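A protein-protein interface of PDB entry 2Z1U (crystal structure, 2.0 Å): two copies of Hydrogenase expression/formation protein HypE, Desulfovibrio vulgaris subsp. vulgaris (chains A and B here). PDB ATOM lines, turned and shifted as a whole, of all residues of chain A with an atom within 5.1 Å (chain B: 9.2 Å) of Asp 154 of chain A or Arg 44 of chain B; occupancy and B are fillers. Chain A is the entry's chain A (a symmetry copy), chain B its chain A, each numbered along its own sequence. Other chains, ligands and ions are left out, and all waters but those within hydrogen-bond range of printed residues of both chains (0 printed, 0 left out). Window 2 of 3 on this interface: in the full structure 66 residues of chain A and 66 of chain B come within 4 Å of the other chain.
The guanidinium group (NH1) of Arg 44 of chain B lies within salt-bridge range of the side-chain carboxylate (OD2) of Asp 154 of chain A (3.6 Å).
The backbone carbonyl oxygen (O) of Leu 45 of chain B lies within hydrogen-bond range of the backbone NH (N) of Leu 51 of chain A.
NH2 of Arg 44 of chain B lies within salt-bridge range of OD1 of Asp 46 of chain B (3.1 Å).
The backbone carbonyl oxygen (O) of Pro 50 of chain A lies within hydrogen-bond range of the backbone NH (N) of Ile 151 of chain A (3.0 Å).
CA of Pro 50 of chain A touches O of Leu 45 of chain B, 3.3 Å away.
Pro 50 of chain A touches Asp 46 of chain B.
O of Leu 51 of chain A touches O of Ala 43 of chain B, at 3.5 Å.
Leu 51 of chain A touches Arg 44 of chain B.
O of Ala 43 of chain B touches CA of Ala 52 of chain A (3.3 Å).
CB of Asn 40 of chain B touches CD1 of Leu 85 of chain A (3.8 Å).
Leu 85 of chain A touches Ala 42 of chain B (CD1 to O, 3.6 Å).
Leu 85 of chain A touches Ala 43 of chain B.
Arg 44 of chain B touches Leu 85 of chain A.
Arg 44 of chain B touches Ile 151 of chain A (CG to CD1, 3.7 Å).
Printed residues of chain B within 4 Å of Leu 51 of chain A: Ala 43, Arg 44 and Leu 45.
Printed residues of chain B within 4 Å of Ala 52 of chain A: Ala 43 (3.3 Å).
No residue of chain B comes within 4 Å of Val 153 of chain A.
Of chain B, only Arg 44 (3.6 Å) comes within 4 Å of Asp 154 of chain A.
Leu 36 of chain B touches none of the printed residues of chain A.
Arg 44 of chain B touches just these residues of chain A: Leu 51, Leu 85, Ile 151 and Asp 154.
Of the printed residues of chain A, Asp 46 of chain B touches Pro 50.
The nearest printed residue of chain B that does not touch Ile 151 of chain A is Leu 45 of chain B (5.2 Å).
Of the 10 printed residues of chain A, 6 touch a printed residue of chain B.
Hydrophobic or aromatic side chains of chain A within 4 Å of the printed part of chain B: Leu 51, Leu 85 and Ile 151.
Printed residues of chain B that touch a printed residue of chain A: Asn 40, Ala 42, Ala 43, Arg 44, Leu 45 and Asp 46.
Among the printed residues, 12 pairs touch across the chains.
No position is printed for both chains.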
ATOM      1  N   PRO A  50      22.829 -25.396  12.444  1.00  0.00           N
ATOM      2  CA  PRO A  50      23.117 -25.512  11.015  1.00  0.00           C
ATOM      3  C   PRO A  50      22.803 -24.175  10.359  1.00  0.00           C
ATOM      4  O   PRO A  50      21.668 -23.699  10.437  1.00  0.00           O
ATOM      5  CB  PRO A  50      22.157 -26.609  10.533  1.00  0.00           C
ATOM      6  CG  PRO A  50      21.533 -27.188  11.780  1.00  0.00           C
ATOM      7  CD  PRO A  50      21.610 -26.123  12.824  1.00  0.00           C
ATOM      8  N   LEU A  51      23.819 -23.563   9.756  1.00  0.00           N
ATOM      9  CA  LEU A  51      23.692 -22.223   9.197  1.00  0.00           C
ATOM     10  C   LEU A  51      23.983 -22.234   7.714  1.00  0.00           C
ATOM     11  O   LEU A  51      24.653 -23.133   7.213  1.00  0.00           O
ATOM     12  CB  LEU A  51      24.646 -21.247   9.900  1.00  0.00           C
ATOM     13  CG  LEU A  51      24.579 -21.180  11.429  1.00  0.00           C
ATOM     14  CD1 LEU A  51      25.690 -20.316  11.926  1.00  0.00           C
ATOM     15  CD2 LEU A  51      23.234 -20.667  11.920  1.00  0.00           C
ATOM     16  N   ALA A  52      23.469 -21.229   7.016  1.00  0.00           N
ATOM     17  CA  ALA A  52      23.780 -21.022   5.614  1.00  0.00           C
ATOM     18  C   ALA A  52      24.520 -19.679   5.453  1.00  0.00           C
ATOM     19  O   ALA A  52      24.101 -18.671   6.020  1.00  0.00           O
ATOM     20  CB  ALA A  52      22.524 -21.056   4.791  1.00  0.00           C
ATOM     21  N   LEU A  85      19.272 -22.009   0.244  1.00  0.00           N
ATOM     22  CA  LEU A  85      19.581 -23.212   1.012  1.00  0.00           C
ATOM     23  C   LEU A  85      18.502 -23.539   2.048  1.00  0.00           C
ATOM     24  O   LEU A  85      18.761 -24.268   3.006  1.00  0.00           O
ATOM     25  CB  LEU A  85      20.939 -23.073   1.701  1.00  0.00           C
ATOM     26  CG  LEU A  85      21.909 -24.241   1.499  1.00  0.00           C
ATOM     27  CD1 LEU A  85      22.377 -24.304   0.036  1.00  0.00           C
ATOM     28  CD2 LEU A  85      23.103 -24.126   2.450  1.00  0.00           C
ATOM     29  N   ILE A 151      19.368 -22.623   8.906  1.00  0.00           N
ATOM     30  CA  ILE A 151      18.707 -23.597   8.034  1.00  0.00           C
ATOM     31  C   ILE A 151      17.432 -24.117   8.697  1.00  0.00           C
ATOM     32  O   ILE A 151      17.424 -24.424   9.899  1.00  0.00           O
ATOM     33  CB  ILE A 151      19.655 -24.717   7.536  1.00  0.00           C
ATOM     34  CG1 ILE A 151      20.675 -24.122   6.552  1.00  0.00           C
ATOM     35  CG2 ILE A 151      18.865 -25.831   6.831  1.00  0.00           C
ATOM     36  CD1 ILE A 151      21.903 -24.948   6.328  1.00  0.00           C
ATOM     37  N   LEU A 152      16.356 -24.162   7.909  1.00  0.00           N
ATOM     38  CA  LEU A 152      15.010 -24.437   8.419  1.00  0.00           C
ATOM     39  C   LEU A 152      14.576 -25.895   8.298  1.00  0.00           C
ATOM     40  O   LEU A 152      13.633 -26.310   8.961  1.00  0.00           O
ATOM     41  CB  LEU A 152      13.974 -23.538   7.729  1.00  0.00           C
ATOM     42  CG  LEU A 152      14.121 -22.021   7.907  1.00  0.00           C
ATOM     43  CD1 LEU A 152      13.255 -21.292   6.890  1.00  0.00           C
ATOM     44  CD2 LEU A 152      13.779 -21.586   9.333  1.00  0.00           C
ATOM     45  N   VAL A 153      15.252 -26.663   7.446  1.00  0.00           N
ATOM     46  CA  VAL A 153      14.825 -28.039   7.152  1.00  0.00           C
ATOM     47  C   VAL A 153      15.988 -28.981   6.897  1.00  0.00           C
ATOM     48  O   VAL A 153      17.058 -28.555   6.455  1.00  0.00           O
ATOM     49  CB  VAL A 153      13.881 -28.119   5.918  1.00  0.00           C
ATOM     50  CG1 VAL A 153      12.480 -27.665   6.268  1.00  0.00           C
ATOM     51  CG2 VAL A 153      14.442 -27.340   4.723  1.00  0.00           C
ATOM     52  N   ASP A 154      15.754 -30.267   7.170  1.00  0.00           N
ATOM     53  CA  ASP A 154      16.688 -31.327   6.809  1.00  0.00           C
ATOM     54  C   ASP A 154      15.910 -32.507   6.219  1.00  0.00           C
ATOM     55  O   ASP A 154      15.014 -33.037   6.876  1.00  0.00           O
ATOM     56  CB  ASP A 154      17.519 -31.765   8.022  1.00  0.00           C
ATOM     57  CG  ASP A 154      18.806 -32.480   7.627  1.00  0.00           C
ATOM     58  OD1 ASP A 154      18.736 -33.603   7.094  1.00  0.00           O
ATOM     59  OD2 ASP A 154      19.897 -31.921   7.860  1.00  0.00           O
ATOM     60  N   PRO A 155      16.234 -32.907   4.968  1.00  0.00           N
ATOM     61  CA  PRO A 155      17.245 -32.283   4.103  1.00  0.00           C
ATOM     62  C   PRO A 155      16.819 -30.916   3.553  1.00  0.00           C
ATOM     63  O   PRO A 155      15.625 -30.666   3.347  1.00  0.00           O
ATOM     64  CB  PRO A 155      17.398 -33.297   2.963  1.00  0.00           C
ATOM     65  CG  PRO A 155      16.115 -34.022   2.924  1.00  0.00           C
ATOM     66  CD  PRO A 155      15.599 -34.069   4.324  1.00  0.00           C
ATOM     67  N   ALA A 156      17.800 -30.050   3.326  1.00  0.00           N
ATOM     68  CA  ALA A 156      17.578 -28.699   2.814  1.00  0.00           C
ATOM     69  C   ALA A 156      17.733 -28.677   1.287  1.00  0.00           C
ATOM     70  O   ALA A 156      18.291 -29.625   0.716  1.00  0.00           O
ATOM     71  CB  ALA A 156      18.555 -27.737   3.470  1.00  0.00           C
ATOM     72  N   ASN B  33      37.879 -28.194  -0.074  1.00  0.00           N
ATOM     73  CA  ASN B  33      37.114 -28.702   1.065  1.00  0.00           C
ATOM     74  C   ASN B  33      35.690 -29.047   0.627  1.00  0.00           C
ATOM     75  O   ASN B  33      35.192 -28.467  -0.341  1.00  0.00           O
ATOM     76  CB  ASN B  33      37.151 -27.717   2.251  1.00  0.00           C
ATOM     77  CG  ASN B  33      36.343 -26.450   2.002  1.00  0.00           C
ATOM     78  OD1 ASN B  33      35.140 -26.420   2.250  1.00  0.00           O
ATOM     79  ND2 ASN B  33      37.005 -25.399   1.530  1.00  0.00           N
ATOM     80  N   PRO B  34      35.032 -29.996   1.324  1.00  0.00           N
ATOM     81  CA  PRO B  34      33.739 -30.495   0.835  1.00  0.00           C
ATOM     82  C   PRO B  34      32.567 -29.559   1.105  1.00  0.00           C
ATOM     83  O   PRO B  34      31.488 -29.761   0.542  1.00  0.00           O
ATOM     84  CB  PRO B  34      33.558 -31.821   1.582  1.00  0.00           C
ATOM     85  CG  PRO B  34      34.329 -31.660   2.832  1.00  0.00           C
ATOM     86  CD  PRO B  34      35.443 -30.661   2.578  1.00  0.00           C
ATOM     87  N   ILE B  35      32.776 -28.549   1.953  1.00  0.00           N
ATOM     88  CA  ILE B  35      31.759 -27.512   2.159  1.00  0.00           C
ATOM     89  C   ILE B  35      31.673 -26.606   0.936  1.00  0.00           C
ATOM     90  O   ILE B  35      30.595 -26.465   0.367  1.00  0.00           O
ATOM     91  CB  ILE B  35      31.957 -26.692   3.448  1.00  0.00           C
ATOM     92  CG1 ILE B  35      31.996 -27.627   4.667  1.00  0.00           C
ATOM     93  CG2 ILE B  35      30.851 -25.638   3.582  1.00  0.00           C
ATOM     94  CD1 ILE B  35      32.190 -26.910   6.018  1.00  0.00           C
ATOM     95  N   LEU B  36      32.788 -25.992   0.547  1.00  0.00           N
ATOM     96  CA  LEU B  36      32.898 -25.282  -0.742  1.00  0.00           C
ATOM     97  C   LEU B  36      32.521 -26.155  -1.961  1.00  0.00           C
ATOM     98  O   LEU B  36      31.842 -25.689  -2.890  1.00  0.00           O
ATOM     99  CB  LEU B  36      34.331 -24.758  -0.945  1.00  0.00           C
ATOM    100  CG  LEU B  36      34.562 -23.919  -2.208  1.00  0.00           C
ATOM    101  CD1 LEU B  36      33.579 -22.728  -2.278  1.00  0.00           C
ATOM    102  CD2 LEU B  36      36.000 -23.453  -2.296  1.00  0.00           C
ATOM    103  N   GLY B  37      32.977 -27.410  -1.953  1.00  0.00           N
ATOM    104  CA  GLY B  37      32.817 -28.329  -3.101  1.00  0.00           C
ATOM    105  C   GLY B  37      31.363 -28.511  -3.507  1.00  0.00           C
ATOM    106  O   GLY B  37      31.045 -28.841  -4.634  1.00  0.00           O
ATOM    107  N   THR B  38      30.476 -28.261  -2.563  1.00  0.00           N
ATOM    108  CA  THR B  38      29.048 -28.362  -2.773  1.00  0.00           C
ATOM    109  C   THR B  38      28.551 -27.445  -3.936  1.00  0.00           C
ATOM    110  O   THR B  38      27.613 -27.799  -4.667  1.00  0.00           O
ATOM    111  CB  THR B  38      28.373 -28.068  -1.415  1.00  0.00           C
ATOM    112  OG1 THR B  38      27.314 -28.988  -1.185  1.00  0.00           O
ATOM    113  CG2 THR B  38      27.900 -26.672  -1.320  1.00  0.00           C
ATOM    114  N   LEU B  39      29.205 -26.291  -4.123  1.00  0.00           N
ATOM    115  CA  LEU B  39      28.892 -25.362  -5.230  1.00  0.00           C
ATOM    116  C   LEU B  39      27.405 -24.969  -5.287  1.00  0.00           C
ATOM    117  O   LEU B  39      26.779 -24.922  -6.365  1.00  0.00           O
ATOM    118  CB  LEU B  39      29.400 -25.899  -6.584  1.00  0.00           C
ATOM    119  CG  LEU B  39      30.925 -25.938  -6.779  1.00  0.00           C
ATOM    120  CD1 LEU B  39      31.303 -26.566  -8.094  1.00  0.00           C
ATOM    121  CD2 LEU B  39      31.510 -24.529  -6.670  1.00  0.00           C
ATOM    122  N   ASN B  40      26.835 -24.726  -4.110  1.00  0.00           N
ATOM    123  CA  ASN B  40      25.465 -24.271  -4.001  1.00  0.00           C
ATOM    124  C   ASN B  40      25.438 -22.748  -3.833  1.00  0.00           C
ATOM    125  O   ASN B  40      26.505 -22.102  -3.778  1.00  0.00           O
ATOM    126  CB  ASN B  40      24.774 -24.962  -2.820  1.00  0.00           C
ATOM    127  CG  ASN B  40      24.380 -26.403  -3.136  1.00  0.00           C
ATOM    128  OD1 ASN B  40      24.417 -27.270  -2.265  1.00  0.00           O
ATOM    129  ND2 ASN B  40      24.008 -26.662  -4.378  1.00  0.00           N
ATOM    130  N   ASP B  41      24.235 -22.180  -3.723  1.00  0.00           N
ATOM    131  CA  ASP B  41      24.085 -20.731  -3.536  1.00  0.00           C
ATOM    132  C   ASP B  41      24.603 -20.242  -2.180  1.00  0.00           C
ATOM    133  O   ASP B  41      24.832 -19.045  -1.994  1.00  0.00           O
ATOM    134  CB  ASP B  41      22.618 -20.346  -3.641  1.00  0.00           C
ATOM    135  CG  ASP B  41      22.077 -20.585  -5.008  1.00  0.00           C
ATOM    136  OD1 ASP B  41      21.411 -21.622  -5.218  1.00  0.00           O
ATOM    137  OD2 ASP B  41      22.340 -19.727  -5.862  1.00  0.00           O
ATOM    138  N   ALA B  42      24.751 -21.171  -1.238  1.00  0.00           N
ATOM    139  CA  ALA B  42      25.343 -20.861   0.061  1.00  0.00           C
ATOM    140  C   ALA B  42      26.071 -22.086   0.582  1.00  0.00           C
ATOM    141  O   ALA B  42      25.808 -23.204   0.141  1.00  0.00           O
ATOM    142  CB  ALA B  42      24.260 -20.404   1.058  1.00  0.00           C
ATOM    143  N   ALA B  43      26.958 -21.858   1.543  1.00  0.00           N
ATOM    144  CA  ALA B  43      27.641 -22.931   2.235  1.00  0.00           C
ATOM    145  C   ALA B  43      26.856 -23.324   3.494  1.00  0.00           C
ATOM    146  O   ALA B  43      26.364 -22.456   4.216  1.00  0.00           O
ATOM    147  CB  ALA B  43      29.053 -22.479   2.602  1.00  0.00           C
ATOM    148  N   ARG B  44      26.760 -24.624   3.753  1.00  0.00           N
ATOM    149  CA  ARG B  44      26.174 -25.144   4.992  1.00  0.00           C
ATOM    150  C   ARG B  44      27.250 -25.258   6.051  1.00  0.00           C
ATOM    151  O   ARG B  44      28.301 -25.875   5.822  1.00  0.00           O
ATOM    152  CB  ARG B  44      25.506 -26.518   4.787  1.00  0.00           C
ATOM    153  CG  ARG B  44      24.956 -27.096   6.085  1.00  0.00           C
ATOM    154  CD  ARG B  44      24.845 -28.602   6.042  1.00  0.00           C
ATOM    155  NE  ARG B  44      24.852 -29.167   7.393  1.00  0.00           N
ATOM    156  CZ  ARG B  44      23.765 -29.593   8.028  1.00  0.00           C
ATOM    157  NH1 ARG B  44      22.575 -29.529   7.431  1.00  0.00           N
ATOM    158  NH2 ARG B  44      23.866 -30.093   9.254  1.00  0.00           N
ATOM    159  N   LEU B  45      26.975 -24.657   7.210  1.00  0.00           N
ATOM    160  CA  LEU B  45      27.920 -24.550   8.306  1.00  0.00           C
ATOM    161  C   LEU B  45      27.334 -25.115   9.608  1.00  0.00           C
ATOM    162  O   LEU B  45      26.202 -24.799   9.981  1.00  0.00           O
ATOM    163  CB  LEU B  45      28.290 -23.073   8.495  1.00  0.00           C
ATOM    164  CG  LEU B  45      29.503 -22.423   7.817  1.00  0.00           C
ATOM    165  CD1 LEU B  45      29.927 -23.009   6.478  1.00  0.00           C
ATOM    166  CD2 LEU B  45      29.331 -20.931   7.739  1.00  0.00           C
ATOM    167  N   ASP B  46      28.099 -25.952  10.300  1.00  0.00           N
ATOM    168  CA  ASP B  46      27.691 -26.417  11.626  1.00  0.00           C
ATOM    169  C   ASP B  46      28.483 -25.710  12.696  1.00  0.00           C
ATOM    170  O   ASP B  46      29.618 -26.091  12.961  1.00  0.00           O
ATOM    171  CB  ASP B  46      27.902 -27.925  11.763  1.00  0.00           C
ATOM    172  CG  ASP B  46      26.945 -28.709  10.945  1.00  0.00           C
ATOM    173  OD1 ASP B  46      25.718 -28.486  11.089  1.00  0.00           O
ATOM    174  OD2 ASP B  46      27.419 -29.552  10.157  1.00  0.00           O
ATOM    175  N   LEU B  47      27.886 -24.701  13.327  1.00  0.00           N
ATOM    176  CA  LEU B  47      28.619 -23.879  14.303  1.00  0.00           C
ATOM    177  C   LEU B  47      27.981 -23.724  15.698  1.00  0.00           C
ATOM    178  O   LEU B  47      26.755 -23.693  15.839  1.00  0.00           O
ATOM    179  CB  LEU B  47      28.927 -22.499  13.707  1.00  0.00           C
ATOM    180  CG  LEU B  47      29.989 -22.402  12.613  1.00  0.00           C
ATOM    181  CD1 LEU B  47      29.915 -21.037  11.931  1.00  0.00           C
ATOM    182  CD2 LEU B  47      31.376 -22.634  13.186  1.00  0.00           C
ATOM    183  N   TYR B  91      35.535 -20.305   9.426  1.00  0.00           N
ATOM    184  CA  TYR B  91      35.100 -20.294   8.019  1.00  0.00           C
ATOM    185  C   TYR B  91      35.134 -18.917   7.416  1.00  0.00           C
ATOM    186  O   TYR B  91      34.691 -17.957   8.036  1.00  0.00           O
ATOM    187  CB  TYR B  91      33.678 -20.863   7.876  1.00  0.00           C
ATOM    188  CG  TYR B  91      33.534 -22.284   8.395  1.00  0.00           C
ATOM    189  CD1 TYR B  91      34.278 -23.326   7.831  1.00  0.00           C
ATOM    190  CD2 TYR B  91      32.668 -22.583   9.447  1.00  0.00           C
ATOM    191  CE1 TYR B  91      34.160 -24.632   8.285  1.00  0.00           C
ATOM    192  CE2 TYR B  91      32.539 -23.887   9.910  1.00  0.00           C
ATOM    193  CZ  TYR B  91      33.286 -24.907   9.324  1.00  0.00           C
ATOM    194  OH  TYR B  91      33.169 -26.200   9.790  1.00  0.00           O
ATOM    195  N   VAL B 126      34.777 -21.324   2.472  1.00  0.00           N
ATOM    196  CA  VAL B 126      33.592 -22.185   2.260  1.00  0.00           C
ATOM    197  C   VAL B 126      32.639 -21.741   1.165  1.00  0.00           C
ATOM    198  O   VAL B 126      31.795 -22.522   0.729  1.00  0.00           O
ATOM    199  CB  VAL B 126      32.767 -22.397   3.575  1.00  0.00           C
ATOM    200  CG1 VAL B 126      33.601 -23.168   4.609  1.00  0.00           C
ATOM    201  CG2 VAL B 126      32.235 -21.039   4.152  1.00  0.00           C
ATOM    202  N   THR B 127      32.755 -20.487   0.736  1.00  0.00           N
ATOM    203  CA  THR B 127      31.793 -19.917  -0.216  1.00  0.00           C
ATOM    204  C   THR B 127      32.424 -18.653  -0.813  1.00  0.00           C
ATOM    205  O   THR B 127      33.297 -18.046  -0.208  1.00  0.00           O
ATOM    206  CB  THR B 127      30.395 -19.635   0.459  1.00  0.00           C
ATOM    207  OG1 THR B 127      29.363 -19.493  -0.535  1.00  0.00           O
ATOM    208  CG2 THR B 127      30.418 -18.387   1.357  1.00  0.00           C
ATOM    209  N   ILE B 148      33.753 -16.040  10.006  1.00  0.00           N
ATOM    210  CA  ILE B 148      32.856 -16.455  11.059  1.00  0.00           C
ATOM    211  C   ILE B 148      33.591 -17.385  12.029  1.00  0.00           C
ATOM    212  O   ILE B 148      34.271 -18.331  11.614  1.00  0.00           O
ATOM    213  CB  ILE B 148      31.554 -17.098  10.476  1.00  0.00           C
ATOM    214  CG1 ILE B 148      30.488 -17.248  11.560  1.00  0.00           C
ATOM    215  CG2 ILE B 148      31.828 -18.428   9.791  1.00  0.00           C
ATOM    216  CD1 ILE B 148      29.554 -16.037  11.600  1.00  0.00           C
